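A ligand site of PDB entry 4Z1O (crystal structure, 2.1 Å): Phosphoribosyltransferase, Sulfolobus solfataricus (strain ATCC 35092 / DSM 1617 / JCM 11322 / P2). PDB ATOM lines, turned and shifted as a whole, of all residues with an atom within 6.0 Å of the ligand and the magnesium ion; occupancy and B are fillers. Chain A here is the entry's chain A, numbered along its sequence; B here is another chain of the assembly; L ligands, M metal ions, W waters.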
ATOM      1  N   VAL A  36     -19.255 -22.563   8.445  1.00  0.00           N
ATOM      2  CA  VAL A  36     -17.846 -22.760   8.101  1.00  0.00           C
ATOM      3  C   VAL A  36     -17.362 -23.982   8.866  1.00  0.00           C
ATOM      4  O   VAL A  36     -17.237 -23.945  10.088  1.00  0.00           O
ATOM      5  CB  VAL A  36     -16.976 -21.528   8.439  1.00  0.00           C
ATOM      6  CG1 VAL A  36     -15.507 -21.737   7.997  1.00  0.00           C
ATOM      7  CG2 VAL A  36     -17.558 -20.280   7.783  1.00  0.00           C
ATOM      8  N   LEU A  37     -17.140 -25.075   8.147  1.00  0.00           N
ATOM      9  CA  LEU A  37     -16.700 -26.313   8.790  1.00  0.00           C
ATOM     10  C   LEU A  37     -15.245 -26.163   9.256  1.00  0.00           C
ATOM     11  O   LEU A  37     -14.443 -25.539   8.561  1.00  0.00           O
ATOM     12  CB  LEU A  37     -16.813 -27.497   7.829  1.00  0.00           C
ATOM     13  CG  LEU A  37     -18.154 -27.815   7.162  1.00  0.00           C
ATOM     14  CD1 LEU A  37     -18.012 -29.015   6.215  1.00  0.00           C
ATOM     15  CD2 LEU A  37     -19.240 -28.070   8.179  1.00  0.00           C
ATOM     16  N   THR A  38     -14.902 -26.719  10.421  1.00  0.00           N
ATOM     17  CA  THR A  38     -15.834 -27.430  11.310  1.00  0.00           C
ATOM     18  C   THR A  38     -16.110 -26.611  12.567  1.00  0.00           C
ATOM     19  O   THR A  38     -16.945 -26.970  13.394  1.00  0.00           O
ATOM     20  CB  THR A  38     -15.284 -28.816  11.716  1.00  0.00           C
ATOM     21  OG1 THR A  38     -14.021 -28.652  12.379  1.00  0.00           O
ATOM     22  CG2 THR A  38     -15.089 -29.708  10.522  1.00  0.00           C
ATOM     23  N   GLY A  39     -15.380 -25.518  12.727  1.00  0.00           N
ATOM     24  CA  GLY A  39     -15.515 -24.685  13.913  1.00  0.00           C
ATOM     25  C   GLY A  39     -16.815 -23.901  13.961  1.00  0.00           C
ATOM     26  O   GLY A  39     -17.301 -23.590  15.050  1.00  0.00           O
ATOM     27  N   GLY A  40     -17.376 -23.567  12.805  1.00  0.00           N
ATOM     28  CA  GLY A  40     -18.616 -22.794  12.756  1.00  0.00           C
ATOM     29  C   GLY A  40     -19.844 -23.681  12.781  1.00  0.00           C
ATOM     30  O   GLY A  40     -20.976 -23.220  12.578  1.00  0.00           O
ATOM     31  N   ILE A  61     -13.533 -26.036   4.450  1.00  0.00           N
ATOM     32  CA  ILE A  61     -12.363 -25.201   4.245  1.00  0.00           C
ATOM     33  C   ILE A  61     -11.427 -25.305   5.462  1.00  0.00           C
ATOM     34  O   ILE A  61     -11.872 -25.391   6.610  1.00  0.00           O
ATOM     35  CB  ILE A  61     -12.787 -23.727   3.974  1.00  0.00           C
ATOM     36  CG1 ILE A  61     -11.581 -22.841   3.671  1.00  0.00           C
ATOM     37  CG2 ILE A  61     -13.576 -23.166   5.139  1.00  0.00           C
ATOM     38  CD1 ILE A  61     -11.956 -21.425   3.289  1.00  0.00           C
ATOM     39  N   LYS A  62     -10.121 -25.325   5.223  1.00  0.00           N
ATOM     40  CA  LYS A  62      -9.196 -25.294   6.344  1.00  0.00           C
ATOM     41  C   LYS A  62      -7.982 -24.401   6.100  1.00  0.00           C
ATOM     42  O   LYS A  62      -7.470 -24.273   4.979  1.00  0.00           O
ATOM     43  CB  LYS A  62      -8.735 -26.710   6.718  1.00  0.00           C
ATOM     44  CG  LYS A  62      -8.928 -26.986   8.207  1.00  0.00           C
ATOM     45  CD  LYS A  62      -8.161 -28.205   8.702  1.00  0.00           C
ATOM     46  CE  LYS A  62      -6.677 -27.913   8.883  1.00  0.00           C
ATOM     47  NZ  LYS A  62      -5.914 -29.160   9.223  1.00  0.00           N
ATOM     48  N   PHE A  63      -7.550 -23.773   7.186  1.00  0.00           N
ATOM     49  CA  PHE A  63      -6.380 -22.915   7.185  1.00  0.00           C
ATOM     50  C   PHE A  63      -5.299 -23.604   8.005  1.00  0.00           C
ATOM     51  O   PHE A  63      -5.298 -23.498   9.225  1.00  0.00           O
ATOM     52  CB  PHE A  63      -6.740 -21.530   7.736  1.00  0.00           C
ATOM     53  CG  PHE A  63      -5.765 -20.437   7.372  1.00  0.00           C
ATOM     54  CD1 PHE A  63      -4.752 -20.657   6.444  1.00  0.00           C
ATOM     55  CD2 PHE A  63      -5.873 -19.180   7.947  1.00  0.00           C
ATOM     56  CE1 PHE A  63      -3.867 -19.664   6.108  1.00  0.00           C
ATOM     57  CE2 PHE A  63      -4.997 -18.171   7.624  1.00  0.00           C
ATOM     58  CZ  PHE A  63      -3.983 -18.409   6.695  1.00  0.00           C
ATOM     59  N   TYR A  64      -4.422 -24.334   7.320  1.00  0.00           N
ATOM     60  CA  TYR A  64      -3.317 -25.031   7.965  1.00  0.00           C
ATOM     61  C   TYR A  64      -2.364 -24.076   8.677  1.00  0.00           C
ATOM     62  O   TYR A  64      -1.804 -23.170   8.062  1.00  0.00           O
ATOM     63  CB  TYR A  64      -2.523 -25.860   6.953  1.00  0.00           C
ATOM     64  CG  TYR A  64      -3.229 -27.111   6.477  1.00  0.00           C
ATOM     65  CD1 TYR A  64      -3.239 -28.262   7.246  1.00  0.00           C
ATOM     66  CD2 TYR A  64      -3.873 -27.141   5.243  1.00  0.00           C
ATOM     67  CE1 TYR A  64      -3.884 -29.415   6.817  1.00  0.00           C
ATOM     68  CE2 TYR A  64      -4.510 -28.275   4.805  1.00  0.00           C
ATOM     69  CZ  TYR A  64      -4.523 -29.404   5.592  1.00  0.00           C
ATOM     70  OH  TYR A  64      -5.160 -30.539   5.153  1.00  0.00           O
ATOM     71  N   ARG A  65      -2.193 -24.287   9.979  1.00  0.00           N
ATOM     72  CA  ARG A  65      -1.255 -23.491  10.766  1.00  0.00           C
ATOM     73  C   ARG A  65      -0.646 -24.335  11.886  1.00  0.00           C
ATOM     74  O   ARG A  65       0.442 -24.901  11.721  1.00  0.00           O
ATOM     75  CB  ARG A  65      -1.954 -22.262  11.361  1.00  0.00           C
ATOM     76  CG  ARG A  65      -2.212 -21.129  10.363  1.00  0.00           C
ATOM     77  CD  ARG A  65      -3.064 -20.026  10.974  1.00  0.00           C
ATOM     78  NE  ARG A  65      -4.450 -20.448  11.161  1.00  0.00           N
ATOM     79  CZ  ARG A  65      -5.490 -19.609  11.219  1.00  0.00           C
ATOM     80  NH1 ARG A  65      -5.289 -18.306  11.104  1.00  0.00           N
ATOM     81  NH2 ARG A  65      -6.716 -20.084  11.384  1.00  0.00           N
ATOM     82  N   PRO A  74      -6.067 -20.288   3.354  1.00  0.00           N
ATOM     83  CA  PRO A  74      -7.081 -21.313   3.576  1.00  0.00           C
ATOM     84  C   PRO A  74      -7.307 -22.104   2.286  1.00  0.00           C
ATOM     85  O   PRO A  74      -7.095 -21.572   1.201  1.00  0.00           O
ATOM     86  CB  PRO A  74      -8.324 -20.509   3.974  1.00  0.00           C
ATOM     87  CG  PRO A  74      -8.057 -19.108   3.499  1.00  0.00           C
ATOM     88  CD  PRO A  74      -6.576 -18.922   3.551  1.00  0.00           C
ATOM     89  N   ARG A  77     -11.919 -27.446   0.406  1.00  0.00           N
ATOM     90  CA  ARG A  77     -11.875 -28.840   0.038  1.00  0.00           C
ATOM     91  C   ARG A  77     -13.231 -29.274  -0.506  1.00  0.00           C
ATOM     92  O   ARG A  77     -13.302 -30.125  -1.404  1.00  0.00           O
ATOM     93  CB  ARG A  77     -11.452 -29.673   1.235  1.00  0.00           C
ATOM     94  CG  ARG A  77     -10.083 -29.191   1.767  1.00  0.00           C
ATOM     95  CD  ARG A  77      -9.512 -30.053   2.857  1.00  0.00           C
ATOM     96  NE  ARG A  77     -10.354 -30.106   4.048  1.00  0.00           N
ATOM     97  CZ  ARG A  77      -9.882 -30.243   5.287  1.00  0.00           C
ATOM     98  NH1 ARG A  77      -8.561 -30.317   5.489  1.00  0.00           N
ATOM     99  NH2 ARG A  77     -10.714 -30.294   6.310  1.00  0.00           N
ATOM    100  N   ASP A  93     -19.166 -18.489  11.520  1.00  0.00           N
ATOM    101  CA  ASP A  93     -17.942 -19.151  11.965  1.00  0.00           C
ATOM    102  C   ASP A  93     -17.758 -18.948  13.450  1.00  0.00           C
ATOM    103  O   ASP A  93     -18.501 -18.192  14.060  1.00  0.00           O
ATOM    104  CB  ASP A  93     -16.727 -18.636  11.176  1.00  0.00           C
ATOM    105  CG  ASP A  93     -15.602 -19.644  11.124  1.00  0.00           C
ATOM    106  OD1 ASP A  93     -15.665 -20.613  11.912  1.00  0.00           O
ATOM    107  OD2 ASP A  93     -14.679 -19.483  10.292  1.00  0.00           O
ATOM    108  N   ASP A  94     -16.792 -19.631  14.058  1.00  0.00           N
ATOM    109  CA  ASP A  94     -16.622 -19.524  15.512  1.00  0.00           C
ATOM    110  C   ASP A  94     -15.704 -18.359  15.903  1.00  0.00           C
ATOM    111  O   ASP A  94     -15.949 -17.673  16.904  1.00  0.00           O
ATOM    112  CB  ASP A  94     -16.094 -20.846  16.103  1.00  0.00           C
ATOM    113  CG  ASP A  94     -14.815 -21.370  15.434  1.00  0.00           C
ATOM    114  OD1 ASP A  94     -14.392 -20.851  14.376  1.00  0.00           O
ATOM    115  OD2 ASP A  94     -14.229 -22.330  15.980  1.00  0.00           O
ATOM    116  N   VAL A  95     -14.654 -18.137  15.117  1.00  0.00           N
ATOM    117  CA  VAL A  95     -13.748 -17.011  15.354  1.00  0.00           C
ATOM    118  C   VAL A  95     -13.114 -16.501  14.053  1.00  0.00           C
ATOM    119  O   VAL A  95     -12.816 -17.290  13.138  1.00  0.00           O
ATOM    120  CB  VAL A  95     -12.607 -17.394  16.360  1.00  0.00           C
ATOM    121  CG1 VAL A  95     -11.667 -18.460  15.774  1.00  0.00           C
ATOM    122  CG2 VAL A  95     -11.811 -16.152  16.795  1.00  0.00           C
ATOM    123  N   ALA A  96     -12.931 -15.184  13.962  1.00  0.00           N
ATOM    124  CA  ALA A  96     -12.112 -14.598  12.907  1.00  0.00           C
ATOM    125  C   ALA A  96     -10.735 -14.175  13.456  1.00  0.00           C
ATOM    126  O   ALA A  96     -10.618 -13.180  14.178  1.00  0.00           O
ATOM    127  CB  ALA A  96     -12.827 -13.415  12.253  1.00  0.00           C
ATOM    128  N   ASP A  97      -9.705 -14.943  13.103  1.00  0.00           N
ATOM    129  CA  ASP A  97      -8.349 -14.708  13.595  1.00  0.00           C
ATOM    130  C   ASP A  97      -7.621 -13.728  12.699  1.00  0.00           C
ATOM    131  O   ASP A  97      -7.599 -12.533  12.993  1.00  0.00           O
ATOM    132  CB  ASP A  97      -7.571 -16.030  13.675  1.00  0.00           C
ATOM    133  CG  ASP A  97      -6.287 -15.903  14.505  1.00  0.00           C
ATOM    134  OD1 ASP A  97      -5.723 -14.798  14.625  1.00  0.00           O
ATOM    135  OD2 ASP A  97      -5.837 -16.945  15.040  1.00  0.00           O
ATOM    136  N   THR A  98      -7.042 -14.208  11.604  1.00  0.00           N
ATOM    137  CA  THR A  98      -6.471 -13.315  10.610  1.00  0.00           C
ATOM    138  C   THR A  98      -7.555 -12.785   9.681  1.00  0.00           C
ATOM    139  O   THR A  98      -7.378 -11.731   9.064  1.00  0.00           O
ATOM    140  CB  THR A  98      -5.408 -13.986   9.750  1.00  0.00           C
ATOM    141  OG1 THR A  98      -6.048 -14.851   8.792  1.00  0.00           O
ATOM    142  CG2 THR A  98      -4.427 -14.760  10.611  1.00  0.00           C
ATOM    143  N   GLY A  99      -8.663 -13.527   9.574  1.00  0.00           N
ATOM    144  CA  GLY A  99      -9.777 -13.127   8.729  1.00  0.00           C
ATOM    145  C   GLY A  99      -9.717 -13.707   7.320  1.00  0.00           C
ATOM    146  O   GLY A  99     -10.649 -13.498   6.521  1.00  0.00           O
ATOM    147  N   GLU A 100      -8.636 -14.411   7.011  1.00  0.00           N
ATOM    148  CA  GLU A 100      -8.499 -15.121   5.746  1.00  0.00           C
ATOM    149  C   GLU A 100      -9.678 -16.065   5.449  1.00  0.00           C
ATOM    150  O   GLU A 100     -10.221 -16.076   4.342  1.00  0.00           O
ATOM    151  CB  GLU A 100      -7.187 -15.930   5.729  1.00  0.00           C
ATOM    152  CG  GLU A 100      -5.944 -15.096   5.437  1.00  0.00           C
ATOM    153  CD  GLU A 100      -5.883 -14.633   3.981  1.00  0.00           C
ATOM    154  OE1 GLU A 100      -6.140 -15.470   3.083  1.00  0.00           O
ATOM    155  OE2 GLU A 100      -5.602 -13.431   3.745  1.00  0.00           O
ATOM    156  N   THR A 101     -10.061 -16.865   6.440  1.00  0.00           N
ATOM    157  CA  THR A 101     -11.135 -17.824   6.243  1.00  0.00           C
ATOM    158  C   THR A 101     -12.460 -17.139   5.877  1.00  0.00           C
ATOM    159  O   THR A 101     -13.069 -17.481   4.865  1.00  0.00           O
ATOM    160  CB  THR A 101     -11.311 -18.716   7.484  1.00  0.00           C
ATOM    161  OG1 THR A 101     -10.168 -19.575   7.612  1.00  0.00           O
ATOM    162  CG2 THR A 101     -12.569 -19.550   7.355  1.00  0.00           C
ATOM    163  N   LEU A 102     -12.882 -16.137   6.651  1.00  0.00           N
ATOM    164  CA  LEU A 102     -14.125 -15.444   6.310  1.00  0.00           C
ATOM    165  C   LEU A 102     -14.054 -14.773   4.940  1.00  0.00           C
ATOM    166  O   LEU A 102     -15.044 -14.731   4.219  1.00  0.00           O
ATOM    167  CB  LEU A 102     -14.505 -14.417   7.370  1.00  0.00           C
ATOM    168  CG  LEU A 102     -15.356 -14.894   8.555  1.00  0.00           C
ATOM    169  CD1 LEU A 102     -15.835 -13.708   9.390  1.00  0.00           C
ATOM    170  CD2 LEU A 102     -16.525 -15.762   8.126  1.00  0.00           C
ATOM    171  N   SER A 128      -7.620  -8.972  12.998  1.00  0.00           N
ATOM    172  CA  SER A 128      -8.304  -9.538  11.844  1.00  0.00           C
ATOM    173  C   SER A 128      -8.312  -8.602  10.642  1.00  0.00           C
ATOM    174  O   SER A 128      -8.515  -7.394  10.776  1.00  0.00           O
ATOM    175  CB  SER A 128      -9.735  -9.929  12.186  1.00  0.00           C
ATOM    176  OG  SER A 128     -10.315 -10.636  11.116  1.00  0.00           O
ATOM    177  N   LYS B  45     -19.159 -33.179  16.034  1.00  0.00           N
ATOM    178  CA  LYS B  45     -18.048 -32.254  16.166  1.00  0.00           C
ATOM    179  C   LYS B  45     -17.305 -32.528  17.477  1.00  0.00           C
ATOM    180  O   LYS B  45     -16.075 -32.591  17.511  1.00  0.00           O
ATOM    181  CB  LYS B  45     -18.526 -30.794  16.090  1.00  0.00           C
ATOM    182  CG  LYS B  45     -17.446 -29.758  16.406  1.00  0.00           C
ATOM    183  CD  LYS B  45     -16.218 -29.875  15.488  1.00  0.00           C
ATOM    184  CE  LYS B  45     -15.183 -28.809  15.827  1.00  0.00           C
ATOM    185  NZ  LYS B  45     -13.920 -28.907  14.980  1.00  0.00           N
HETATM  186  C1  LIG L   1     -10.225 -21.944  12.191  1.00  0.00           C
HETATM  187  C2  LIG L   1     -11.442 -21.345  12.704  1.00  0.00           C
HETATM  188  C3  LIG L   1     -11.832 -20.441  11.636  1.00  0.00           C
HETATM  189  C4  LIG L   1     -10.545 -20.023  11.019  1.00  0.00           C
HETATM  190  C5  LIG L   1     -10.305 -18.572  11.308  1.00  0.00           C
HETATM  191  O1  LIG L   1     -10.555 -22.896  11.296  1.00  0.00           O
HETATM  192  O2  LIG L   1     -12.435 -22.315  12.975  1.00  0.00           O
HETATM  193  O3  LIG L   1     -12.605 -21.051  10.676  1.00  0.00           O
HETATM  194  O4  LIG L   1      -9.544 -20.844  11.564  1.00  0.00           O
HETATM  195  O5  LIG L   1      -9.005 -18.127  11.332  1.00  0.00           O
HETATM  196  P1  LIG L   1      -8.544 -17.104  10.233  1.00  0.00           P
HETATM  197  O6  LIG L   1      -9.449 -15.896  10.337  1.00  0.00           O
HETATM  198  O7  LIG L   1      -7.124 -16.738  10.525  1.00  0.00           O
HETATM  199  O8  LIG L   1      -8.633 -17.704   8.836  1.00  0.00           O
HETATM  200  P2  LIG L   1      -9.577 -24.030  10.929  1.00  0.00           P
HETATM  201  O9  LIG L   1      -8.623 -24.202  12.064  1.00  0.00           O
HETATM  202  O10 LIG L   1      -8.817 -23.725   9.658  1.00  0.00           O
HETATM  203  O11 LIG L   1     -10.375 -25.371  10.700  1.00  0.00           O
HETATM  204  P3  LIG L   1     -11.446 -25.909  11.702  1.00  0.00           P
HETATM  205  O12 LIG L   1     -12.627 -24.951  11.761  1.00  0.00           O
HETATM  206  O13 LIG L   1     -11.917 -27.279  11.204  1.00  0.00           O
HETATM  207  O14 LIG L   1     -10.843 -26.012  13.109  1.00  0.00           O
HETATM  208 MG    MG M   1     -12.759 -23.084  11.014  1.00  0.00          MG
HETATM  209  O   HOH W   1     -11.798 -15.683   9.258  1.00  0.00           O
HETATM  210  O   HOH W   2     -12.335 -26.246  15.263  1.00  0.00           O
HETATM  211  O   HOH W   3     -12.557 -23.475   9.170  1.00  0.00           O
HETATM  212  O   HOH W   4     -10.333 -29.156  10.875  1.00  0.00           O
HETATM  213  O   HOH W   5     -10.548 -22.475   7.410  1.00  0.00           O
HETATM  214  O   HOH W   6     -14.772 -22.945  11.233  1.00  0.00           O
HETATM  215  O   HOH W   7      -9.622 -24.095  14.893  1.00  0.00           O
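The backbone NH (N) of Glu 100 sits at hydrogen-bond distance from the side-chain hydroxyl (OG1) of Thr 98 (3.2 Å). The side-chain hydroxyl of Thr 38 sits at hydrogen-bond distance from the side-chain amino group of Lys 45 of chain B (2.6 Å).
O of Leu 37 touches the magnesium ion, at 3.9 Å. Gly 39 touches the magnesium ion (N to MG, 3.97 Å). OD1 of Asp 93 touches the magnesium ion, 3.9 Å away. Of the 24 residues printed, 3 come within 4 Å of the magnesium ion.
Water W6 lies within hydrogen-bond range of OD1 of Asp 93 (2.6 Å), O of Val 36 (2.9 Å), N of Gly 39 (3.0 Å) and N of Gly 40 (3.1 Å). Water W1 bridges O6 of the ligand and N of Leu 102. Water W2 lies within hydrogen-bond range of O14 of the ligand (2.6 Å) and NZ of Lys 45 of chain B (3.1 Å). Water W5 lies within hydrogen-bond range of the side-chain hydroxyl (OG1) of Thr 101 (2.9 Å), an oxygen (O10) of the ligand (3.1 Å), the backbone NH (N) of Phe 63 (3.3 Å) and the backbone carbonyl oxygen (O) of Ile 61 (3.3 Å).
The guanidinium group (NH1) of Arg 65 is in salt-bridge range of an oxygen (O7) of the ligand, at 2.5 Å. O6 of the ligand sits at hydrogen-bond distance from N of Gly 99. OD2 of Asp 93 sits close to O3 of the ligand (2.6 Å). N of Thr 101 sits at hydrogen-bond distance from O8 of the ligand. The side-chain hydroxyl (OG1) of Thr 101 lies within hydrogen-bond range of an oxygen (O8) of the ligand, at 2.7 Å. An oxygen (O7) of the ligand sits at hydrogen-bond distance from the backbone NH (N) of Thr 98 (2.8 Å). OG1 of Thr 98 sits at hydrogen-bond distance from O7 of the ligand (2.8 Å). The backbone NH of Thr 38 sits at hydrogen-bond distance from an oxygen (O13) of the ligand, at 3.1 Å. OG1 of Thr 38 lies within hydrogen-bond range of O13 of the ligand, 2.8 Å away. The backbone NH (N) of Phe 63 is in hydrogen-bond range of an oxygen (O10) of the ligand. The side-chain carboxylate (OD1) of Asp 94 lies close to an oxygen (O2) of the ligand, 2.8 Å away. N of Asp 97 lies within hydrogen-bond range of O6 of the ligand, 2.9 Å away. N of Gly 39 sits close to O12 of the ligand (3.0 Å).
O of Leu 37 touches O12 of the ligand, at 3.7 Å. CG of Lys 62 touches O11 of the ligand, at 3.3 Å. Val 95 touches the ligand (O to C5, 3.4 Å). C of Ala 96 touches O6 of the ligand, 3.8 Å away. N of Glu 100 touches O6 of the ligand, 3.7 Å away. Within 4 Å of the ligand: Leu 37, Thr 38, Gly 39, Lys 62, Phe 63, Arg 65, Asp 93, Asp 94, Val 95, Ala 96, Asp 97, Thr 98, Gly 99, Glu 100 and Thr 101.
The magnesium ion is bound by water W3, an oxygen (O12) of the ligand, water W6, an oxygen (O3) of the ligand, an oxygen (O2) of the ligand and an oxygen (O1) of the ligand. The magnesium ion has six donor atoms within binding distance.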
